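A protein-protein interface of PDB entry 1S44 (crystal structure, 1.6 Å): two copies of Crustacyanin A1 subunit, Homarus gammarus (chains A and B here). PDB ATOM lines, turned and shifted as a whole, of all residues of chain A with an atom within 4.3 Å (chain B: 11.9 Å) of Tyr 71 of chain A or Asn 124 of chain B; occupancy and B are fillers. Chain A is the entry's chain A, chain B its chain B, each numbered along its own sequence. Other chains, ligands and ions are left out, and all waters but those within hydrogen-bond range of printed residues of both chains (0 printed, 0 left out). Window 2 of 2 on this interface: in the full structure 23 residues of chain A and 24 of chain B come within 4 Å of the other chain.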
ATOM      1  N   ASN A  42      -6.834   2.300  -2.116  1.00  0.00           N
ATOM      2  CA  ASN A  42      -7.234   3.141  -1.044  1.00  0.00           C
ATOM      3  C   ASN A  42      -7.157   4.613  -1.482  1.00  0.00           C
ATOM      4  O   ASN A  42      -6.106   5.078  -1.819  1.00  0.00           O
ATOM      5  CB  ASN A  42      -6.279   2.810   0.114  1.00  0.00           C
ATOM      6  CG  ASN A  42      -6.665   3.493   1.396  1.00  0.00           C
ATOM      7  OD1 ASN A  42      -6.986   4.695   1.360  1.00  0.00           O
ATOM      8  ND2 ASN A  42      -6.599   2.784   2.521  1.00  0.00           N
ATOM      9  N   PRO A  43      -8.304   5.280  -1.592  1.00  0.00           N
ATOM     10  CA  PRO A  43      -8.318   6.638  -2.078  1.00  0.00           C
ATOM     11  C   PRO A  43      -7.896   7.618  -1.032  1.00  0.00           C
ATOM     12  O   PRO A  43      -7.869   8.830  -1.326  1.00  0.00           O
ATOM     13  CB  PRO A  43      -9.827   6.842  -2.415  1.00  0.00           C
ATOM     14  CG  PRO A  43     -10.554   5.965  -1.517  1.00  0.00           C
ATOM     15  CD  PRO A  43      -9.670   4.745  -1.369  1.00  0.00           C
ATOM     16  N   TYR A  44      -7.504   7.108   0.123  1.00  0.00           N
ATOM     17  CA  TYR A  44      -7.212   8.030   1.257  1.00  0.00           C
ATOM     18  C   TYR A  44      -5.756   8.020   1.655  1.00  0.00           C
ATOM     19  O   TYR A  44      -5.369   8.831   2.520  1.00  0.00           O
ATOM     20  CB  TYR A  44      -8.005   7.665   2.450  1.00  0.00           C
ATOM     21  CG  TYR A  44      -9.458   7.509   2.241  1.00  0.00           C
ATOM     22  CD1 TYR A  44     -10.055   6.281   2.265  1.00  0.00           C
ATOM     23  CD2 TYR A  44     -10.264   8.590   2.086  1.00  0.00           C
ATOM     24  CE1 TYR A  44     -11.389   6.108   2.088  1.00  0.00           C
ATOM     25  CE2 TYR A  44     -11.650   8.435   1.952  1.00  0.00           C
ATOM     26  CZ  TYR A  44     -12.198   7.200   1.895  1.00  0.00           C
ATOM     27  OH  TYR A  44     -13.580   6.995   1.745  1.00  0.00           O
ATOM     28  N   GLN A  45      -4.964   7.072   1.166  1.00  0.00           N
ATOM     29  CA  GLN A  45      -3.557   7.021   1.455  1.00  0.00           C
ATOM     30  C   GLN A  45      -2.850   8.049   0.544  1.00  0.00           C
ATOM     31  O   GLN A  45      -2.717   7.823  -0.635  1.00  0.00           O
ATOM     32  CB  GLN A  45      -3.118   5.580   1.149  1.00  0.00           C
ATOM     33  CG  GLN A  45      -1.647   5.215   1.177  1.00  0.00           C
ATOM     34  CD  GLN A  45      -0.948   5.681   2.434  1.00  0.00           C
ATOM     35  OE1 GLN A  45      -0.795   6.876   2.673  1.00  0.00           O
ATOM     36  NE2 GLN A  45      -0.426   4.707   3.203  1.00  0.00           N
ATOM     37  N   LEU A  46      -2.334   9.110   1.152  1.00  0.00           N
ATOM     38  CA  LEU A  46      -1.624  10.168   0.411  1.00  0.00           C
ATOM     39  C   LEU A  46      -0.173   9.810   0.082  1.00  0.00           C
ATOM     40  O   LEU A  46       0.463  10.429  -0.762  1.00  0.00           O
ATOM     41  CB  LEU A  46      -1.672  11.486   1.154  1.00  0.00           C
ATOM     42  CG  LEU A  46      -3.031  12.181   1.198  1.00  0.00           C
ATOM     43  CD1 LEU A  46      -2.928  13.331   2.171  1.00  0.00           C
ATOM     44  CD2 LEU A  46      -3.506  12.645  -0.198  1.00  0.00           C
ATOM     45  N   GLU A  48       2.273   7.331  -1.464  1.00  0.00           N
ATOM     46  CA  GLU A  48       2.375   6.267  -2.469  1.00  0.00           C
ATOM     47  C   GLU A  48       3.470   5.276  -2.267  1.00  0.00           C
ATOM     48  O   GLU A  48       3.250   4.054  -2.408  1.00  0.00           O
ATOM     49  CB  GLU A  48       2.488   6.878  -3.940  1.00  0.00           C
ATOM     50  CG  GLU A  48       2.577   5.781  -4.996  1.00  0.00           C
ATOM     51  CD  GLU A  48       2.765   6.266  -6.434  1.00  0.00           C
ATOM     52  OE1 GLU A  48       2.407   5.470  -7.341  1.00  0.00           O
ATOM     53  OE2 GLU A  48       3.362   7.334  -6.636  1.00  0.00           O
ATOM     54  N   ILE A  69       6.958   8.756   0.036  1.00  0.00           N
ATOM     55  CA  ILE A  69       6.936   9.528  -1.220  1.00  0.00           C
ATOM     56  C   ILE A  69       5.479   9.716  -1.565  1.00  0.00           C
ATOM     57  O   ILE A  69       4.753   8.779  -1.642  1.00  0.00           O
ATOM     58  CB  ILE A  69       7.739   8.818  -2.303  1.00  0.00           C
ATOM     59  CG1 ILE A  69       9.199   8.587  -1.862  1.00  0.00           C
ATOM     60  CG2 ILE A  69       7.837   9.719  -3.537  1.00  0.00           C
ATOM     61  CD1 ILE A  69      10.086   8.051  -3.013  1.00  0.00           C
ATOM     62  N   ALA A  70       5.015  10.974  -1.630  1.00  0.00           N
ATOM     63  CA  ALA A  70       3.641  11.257  -2.109  1.00  0.00           C
ATOM     64  C   ALA A  70       3.501  10.872  -3.599  1.00  0.00           C
ATOM     65  O   ALA A  70       4.453  10.663  -4.266  1.00  0.00           O
ATOM     66  CB  ALA A  70       3.260  12.726  -1.804  1.00  0.00           C
ATOM     67  N   TYR A  71       2.274  10.933  -4.093  1.00  0.00           N
ATOM     68  CA  TYR A  71       1.974  10.701  -5.495  1.00  0.00           C
ATOM     69  C   TYR A  71       2.552  11.745  -6.454  1.00  0.00           C
ATOM     70  O   TYR A  71       2.682  11.457  -7.617  1.00  0.00           O
ATOM     71  CB  TYR A  71       0.484  10.599  -5.678  1.00  0.00           C
ATOM     72  CG  TYR A  71      -0.068   9.248  -5.220  1.00  0.00           C
ATOM     73  CD1 TYR A  71      -0.510   9.086  -3.917  1.00  0.00           C
ATOM     74  CD2 TYR A  71      -0.101   8.177  -6.052  1.00  0.00           C
ATOM     75  CE1 TYR A  71      -1.070   7.926  -3.470  1.00  0.00           C
ATOM     76  CE2 TYR A  71      -0.618   6.958  -5.627  1.00  0.00           C
ATOM     77  CZ  TYR A  71      -1.086   6.828  -4.327  1.00  0.00           C
ATOM     78  OH  TYR A  71      -1.579   5.638  -3.820  1.00  0.00           O
ATOM     79  N   ASP A  72       2.860  12.949  -5.983  1.00  0.00           N
ATOM     80  CA  ASP A  72       3.652  13.887  -6.844  1.00  0.00           C
ATOM     81  C   ASP A  72       5.162  13.697  -6.727  1.00  0.00           C
ATOM     82  O   ASP A  72       5.983  14.360  -7.354  1.00  0.00           O
ATOM     83  CB  ASP A  72       3.283  15.306  -6.489  1.00  0.00           C
ATOM     84  CG  ASP A  72       3.829  15.747  -5.154  1.00  0.00           C
ATOM     85  OD1 ASP A  72       4.246  14.903  -4.374  1.00  0.00           O
ATOM     86  OD2 ASP A  72       3.892  16.979  -4.817  1.00  0.00           O
ATOM     87  N   GLY A  73       5.596  12.740  -5.931  1.00  0.00           N
ATOM     88  CA  GLY A  73       7.002  12.440  -5.980  1.00  0.00           C
ATOM     89  C   GLY A  73       7.782  13.143  -4.928  1.00  0.00           C
ATOM     90  O   GLY A  73       8.972  12.850  -4.834  1.00  0.00           O
ATOM     91  N   VAL B   6     -18.524  13.029  -5.582  1.00  0.00           N
ATOM     92  CA  VAL B   6     -17.080  12.939  -5.824  1.00  0.00           C
ATOM     93  C   VAL B   6     -16.793  14.054  -6.855  1.00  0.00           C
ATOM     94  O   VAL B   6     -17.201  13.978  -7.996  1.00  0.00           O
ATOM     95  CB  VAL B   6     -16.721  11.594  -6.358  1.00  0.00           C
ATOM     96  CG1 VAL B   6     -15.221  11.457  -6.539  1.00  0.00           C
ATOM     97  CG2 VAL B   6     -17.116  10.512  -5.414  1.00  0.00           C
ATOM     98  N   VAL B   7     -16.116  15.090  -6.397  1.00  0.00           N
ATOM     99  CA  VAL B   7     -15.988  16.329  -7.118  1.00  0.00           C
ATOM    100  C   VAL B   7     -14.536  16.711  -7.395  1.00  0.00           C
ATOM    101  O   VAL B   7     -13.681  16.621  -6.507  1.00  0.00           O
ATOM    102  CB  VAL B   7     -16.610  17.473  -6.358  1.00  0.00           C
ATOM    103  CG1 VAL B   7     -16.649  18.692  -7.238  1.00  0.00           C
ATOM    104  CG2 VAL B   7     -18.020  17.134  -5.828  1.00  0.00           C
ATOM    105  N   PRO B   8     -14.216  17.134  -8.628  1.00  0.00           N
ATOM    106  CA  PRO B   8     -12.821  17.496  -8.896  1.00  0.00           C
ATOM    107  C   PRO B   8     -12.356  18.595  -8.024  1.00  0.00           C
ATOM    108  O   PRO B   8     -13.109  19.535  -7.639  1.00  0.00           O
ATOM    109  CB  PRO B   8     -12.831  17.920 -10.381  1.00  0.00           C
ATOM    110  CG  PRO B   8     -14.077  17.154 -10.987  1.00  0.00           C
ATOM    111  CD  PRO B   8     -15.031  17.095  -9.846  1.00  0.00           C
ATOM    112  N   GLY B   9     -11.054  18.491  -7.738  1.00  0.00           N
ATOM    113  CA  GLY B   9     -10.350  19.478  -6.964  1.00  0.00           C
ATOM    114  C   GLY B   9     -10.333  19.138  -5.511  1.00  0.00           C
ATOM    115  O   GLY B   9     -10.711  18.087  -5.126  1.00  0.00           O
ATOM    116  N   LYS B  10      -9.836  20.067  -4.722  1.00  0.00           N
ATOM    117  CA  LYS B  10      -9.653  19.935  -3.311  1.00  0.00           C
ATOM    118  C   LYS B  10     -10.755  20.571  -2.432  1.00  0.00           C
ATOM    119  O   LYS B  10     -11.452  21.491  -2.826  1.00  0.00           O
ATOM    120  CB  LYS B  10      -8.318  20.594  -2.934  1.00  0.00           C
ATOM    121  CG  LYS B  10      -8.594  22.027  -2.541  1.00  0.00           C
ATOM    122  CD  LYS B  10      -7.483  23.035  -2.411  1.00  0.00           C
ATOM    123  CE  LYS B  10      -8.142  24.354  -2.796  1.00  0.00           C
ATOM    124  NZ  LYS B  10      -7.899  25.493  -1.880  1.00  0.00           N
ATOM    125  N   CYS B  11     -10.941  20.057  -1.217  1.00  0.00           N
ATOM    126  CA  CYS B  11     -11.833  20.765  -0.279  1.00  0.00           C
ATOM    127  C   CYS B  11     -11.516  22.272  -0.199  1.00  0.00           C
ATOM    128  O   CYS B  11     -10.359  22.685  -0.058  1.00  0.00           O
ATOM    129  CB  CYS B  11     -11.792  20.159   1.134  1.00  0.00           C
ATOM    130  SG  CYS B  11     -12.355  18.421   1.150  1.00  0.00           S
ATOM    131  N   CYS B 120     -16.086  17.563   4.528  1.00  0.00           N
ATOM    132  CA  CYS B 120     -15.398  17.363   3.246  1.00  0.00           C
ATOM    133  C   CYS B 120     -14.135  16.567   3.494  1.00  0.00           C
ATOM    134  O   CYS B 120     -13.511  16.716   4.544  1.00  0.00           O
ATOM    135  CB  CYS B 120     -15.079  18.732   2.636  1.00  0.00           C
ATOM    136  SG  CYS B 120     -14.436  18.630   0.917  1.00  0.00           S
ATOM    137  N   ILE B 121     -13.774  15.712   2.517  1.00  0.00           N
ATOM    138  CA  ILE B 121     -12.594  14.873   2.619  1.00  0.00           C
ATOM    139  C   ILE B 121     -11.873  14.983   1.250  1.00  0.00           C
ATOM    140  O   ILE B 121     -12.479  14.888   0.184  1.00  0.00           O
ATOM    141  CB  ILE B 121     -12.912  13.404   2.912  1.00  0.00           C
ATOM    142  CG1 ILE B 121     -11.600  12.555   3.076  1.00  0.00           C
ATOM    143  CG2 ILE B 121     -13.758  12.811   1.864  1.00  0.00           C
ATOM    144  CD1 ILE B 121     -11.375  12.011   4.481  1.00  0.00           C
ATOM    145  N   ASP B 122     -10.572  15.106   1.318  1.00  0.00           N
ATOM    146  CA  ASP B 122      -9.730  15.001   0.132  1.00  0.00           C
ATOM    147  C   ASP B 122      -9.209  13.584  -0.124  1.00  0.00           C
ATOM    148  O   ASP B 122      -8.741  12.818   0.769  1.00  0.00           O
ATOM    149  CB  ASP B 122      -8.556  15.954   0.188  1.00  0.00           C
ATOM    150  CG  ASP B 122      -8.950  17.375   0.134  1.00  0.00           C
ATOM    151  OD1 ASP B 122      -9.482  17.824  -0.886  1.00  0.00           O
ATOM    152  OD2 ASP B 122      -8.690  18.195   1.026  1.00  0.00           O
ATOM    153  N   TYR B 123      -9.294  13.209  -1.376  1.00  0.00           N
ATOM    154  CA  TYR B 123      -8.787  11.978  -1.798  1.00  0.00           C
ATOM    155  C   TYR B 123      -7.369  12.191  -2.310  1.00  0.00           C
ATOM    156  O   TYR B 123      -6.891  13.355  -2.446  1.00  0.00           O
ATOM    157  CB  TYR B 123      -9.655  11.381  -2.915  1.00  0.00           C
ATOM    158  CG  TYR B 123     -11.038  11.035  -2.475  1.00  0.00           C
ATOM    159  CD1 TYR B 123     -12.105  11.550  -3.147  1.00  0.00           C
ATOM    160  CD2 TYR B 123     -11.261  10.137  -1.413  1.00  0.00           C
ATOM    161  CE1 TYR B 123     -13.371  11.257  -2.793  1.00  0.00           C
ATOM    162  CE2 TYR B 123     -12.575   9.777  -1.039  1.00  0.00           C
ATOM    163  CZ  TYR B 123     -13.632  10.310  -1.774  1.00  0.00           C
ATOM    164  OH  TYR B 123     -15.000  10.079  -1.451  1.00  0.00           O
ATOM    165  N   ASN B 124      -6.736  11.039  -2.611  1.00  0.00           N
ATOM    166  CA  ASN B 124      -5.388  10.978  -3.195  1.00  0.00           C
ATOM    167  C   ASN B 124      -5.301  11.126  -4.716  1.00  0.00           C
ATOM    168  O   ASN B 124      -4.191  11.176  -5.275  1.00  0.00           O
ATOM    169  CB  ASN B 124      -4.622   9.755  -2.699  1.00  0.00           C
ATOM    170  CG  ASN B 124      -5.204   8.449  -3.196  1.00  0.00           C
ATOM    171  OD1 ASN B 124      -6.030   8.440  -4.124  1.00  0.00           O
ATOM    172  ND2 ASN B 124      -4.758   7.326  -2.633  1.00  0.00           N
ATOM    173  N   PHE B 125      -6.459  11.190  -5.382  1.00  0.00           N
ATOM    174  CA  PHE B 125      -6.551  11.233  -6.860  1.00  0.00           C
ATOM    175  C   PHE B 125      -7.093  12.607  -7.419  1.00  0.00           C
ATOM    176  O   PHE B 125      -7.615  12.670  -8.523  1.00  0.00           O
ATOM    177  CB  PHE B 125      -7.262   9.968  -7.359  1.00  0.00           C
ATOM    178  CG  PHE B 125      -8.714   9.784  -6.952  1.00  0.00           C
ATOM    179  CD1 PHE B 125      -9.747  10.352  -7.672  1.00  0.00           C
ATOM    180  CD2 PHE B 125      -9.033   9.042  -5.840  1.00  0.00           C
ATOM    181  CE1 PHE B 125     -11.132  10.172  -7.279  1.00  0.00           C
ATOM    182  CE2 PHE B 125     -10.349   8.838  -5.444  1.00  0.00           C
ATOM    183  CZ  PHE B 125     -11.407   9.439  -6.112  1.00  0.00           C
ATOM    184  N   GLY B 126      -6.985  13.707  -6.662  1.00  0.00           N
ATOM    185  CA  GLY B 126      -7.326  14.997  -7.242  1.00  0.00           C
ATOM    186  C   GLY B 126      -8.788  15.363  -7.161  1.00  0.00           C
ATOM    187  O   GLY B 126      -9.300  16.173  -7.949  1.00  0.00           O
ATOM    188  N   TYR B 127      -9.504  14.670  -6.273  1.00  0.00           N
ATOM    189  CA  TYR B 127     -10.945  14.896  -6.036  1.00  0.00           C
ATOM    190  C   TYR B 127     -11.167  15.016  -4.534  1.00  0.00           C
ATOM    191  O   TYR B 127     -10.273  14.611  -3.736  1.00  0.00           O
ATOM    192  CB  TYR B 127     -11.815  13.793  -6.526  1.00  0.00           C
ATOM    193  CG  TYR B 127     -12.031  13.659  -8.032  1.00  0.00           C
ATOM    194  CD1 TYR B 127     -13.235  14.008  -8.634  1.00  0.00           C
ATOM    195  CD2 TYR B 127     -11.015  13.196  -8.821  1.00  0.00           C
ATOM    196  CE1 TYR B 127     -13.434  13.796 -10.031  1.00  0.00           C
ATOM    197  CE2 TYR B 127     -11.167  13.041 -10.192  1.00  0.00           C
ATOM    198  CZ  TYR B 127     -12.372  13.351 -10.787  1.00  0.00           C
ATOM    199  OH  TYR B 127     -12.450  13.172 -12.193  1.00  0.00           O
ATOM    200  N   HIS B 128     -12.367  15.533  -4.181  1.00  0.00           N
ATOM    201  CA  HIS B 128     -12.897  15.534  -2.810  1.00  0.00           C
ATOM    202  C   HIS B 128     -14.316  15.004  -2.785  1.00  0.00           C
ATOM    203  O   HIS B 128     -15.004  14.937  -3.820  1.00  0.00           O
ATOM    204  CB  HIS B 128     -12.842  16.924  -2.158  1.00  0.00           C
ATOM    205  CG  HIS B 128     -13.583  17.973  -2.923  1.00  0.00           C
ATOM    206  ND1 HIS B 128     -14.769  18.568  -2.523  1.00  0.00           N
ATOM    207  CD2 HIS B 128     -13.239  18.575  -4.079  1.00  0.00           C
ATOM    208  CE1 HIS B 128     -15.138  19.450  -3.431  1.00  0.00           C
ATOM    209  NE2 HIS B 128     -14.184  19.516  -4.347  1.00  0.00           N
ATOM    210  N   SER B 129     -14.774  14.584  -1.592  1.00  0.00           N
ATOM    211  CA  SER B 129     -16.176  14.283  -1.359  1.00  0.00           C
ATOM    212  C   SER B 129     -16.678  15.166  -0.275  1.00  0.00           C
ATOM    213  O   SER B 129     -16.009  15.374   0.697  1.00  0.00           O
ATOM    214  CB  SER B 129     -16.462  12.838  -0.997  1.00  0.00           C
ATOM    215  OG  SER B 129     -16.647  12.053  -2.146  1.00  0.00           O
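Asn 42 of chain A touches just one residue of chain B: Asn 124 (2.7 Å).
Pro 43 of chain A touches just these residues of chain B: Tyr 123 (3.3 Å), Asn 124 (2.8 Å) and Phe 125 (3.7 Å).
Gln 45 of chain A touches just one residue of chain B: Asn 124 (2.9 Å).
No residue of chain B comes within 4 Å of Ala 70 of chain A.
No residue of chain B comes within 4 Å of Asp 72 of chain A.
No residue of chain B comes within 4 Å of Gly 73 of chain A.
Ile 121 of chain B touches none of the printed residues of chain A.
Asp 122 of chain B touches none of the printed residues of chain A.
Printed residues of chain A within 4 Å of Tyr 123 of chain B: Pro 43 and Tyr 44.
Of chain A, only Asn 42 (2.7 Å), Pro 43 (2.8 Å), Tyr 44 (3.9 Å), Gln 45 (2.9 Å), Leu 46 (3.9 Å) and Tyr 71 (3.8 Å) come within 4 Å of Asn 124 of chain B.
Of the printed residues of chain A, Phe 125 of chain B touches Pro 43.
Of the 11 printed residues of chain A, 6 touch a printed residue of chain B.
Printed residues of chain A that touch a printed residue of chain B: Asn 42, Pro 43, Tyr 44, Gln 45, Leu 46 and Tyr 71.
Hydrophobic or aromatic side chains of chain A within 4 Å of the printed part of chain B: Pro 43, Tyr 44, Leu 46 and Tyr 71.
Among the printed residues, 9 pairs touch across the chains.
Among the printed residues, no Asp or Glu carboxylate lies within 4 Å of a Lys or Arg side-chain nitrogen of the other chain.
Among the printed residues, merely in contact across the chains: Pro 43 of chain A with Tyr 123 of chain B, Pro 43 of chain A with Phe 125 of chain B, Tyr 44 of chain A with Tyr 123 of chain B, Tyr 44 of chain A with Asn 124 of chain B, Leu 46 of chain A with Asn 124 of chain B and Tyr 71 of chain A with Asn 124 of chain B.
O of Asn 42 of chain A lies within hydrogen-bond range of ND2 of Asn 124 of chain B.
N of Asn 124 of chain B is in hydrogen-bond range of O of Pro 43 of chain A, 2.8 Å away.
ND2 of Asn 124 of chain B is in hydrogen-bond range of O of Gln 45 of chain A (2.9 Å).
The backbone NH of Tyr 44 of chain A is in hydrogen-bond range of the side-chain amide oxygen of Asn 42 of chain A (2.8 Å).
The backbone NH (N) of Gln 45 of chain A is in hydrogen-bond range of the side-chain amide oxygen (OD1) of Asn 42 of chain A (3.1 Å).
OH of Tyr 123 of chain B lies within hydrogen-bond range of OG of Ser 129 of chain B, 2.7 Å away.
The side-chain sulfur of Cys 11 of chain B forms a disulfide with the side-chain sulfur of Cys 120 of chain B, 2.1 Å away.
No position is printed for both chains.
Of the 9 pairs that touch across the chains among the printed residues, none has its exchanged pair printed and touching as well.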
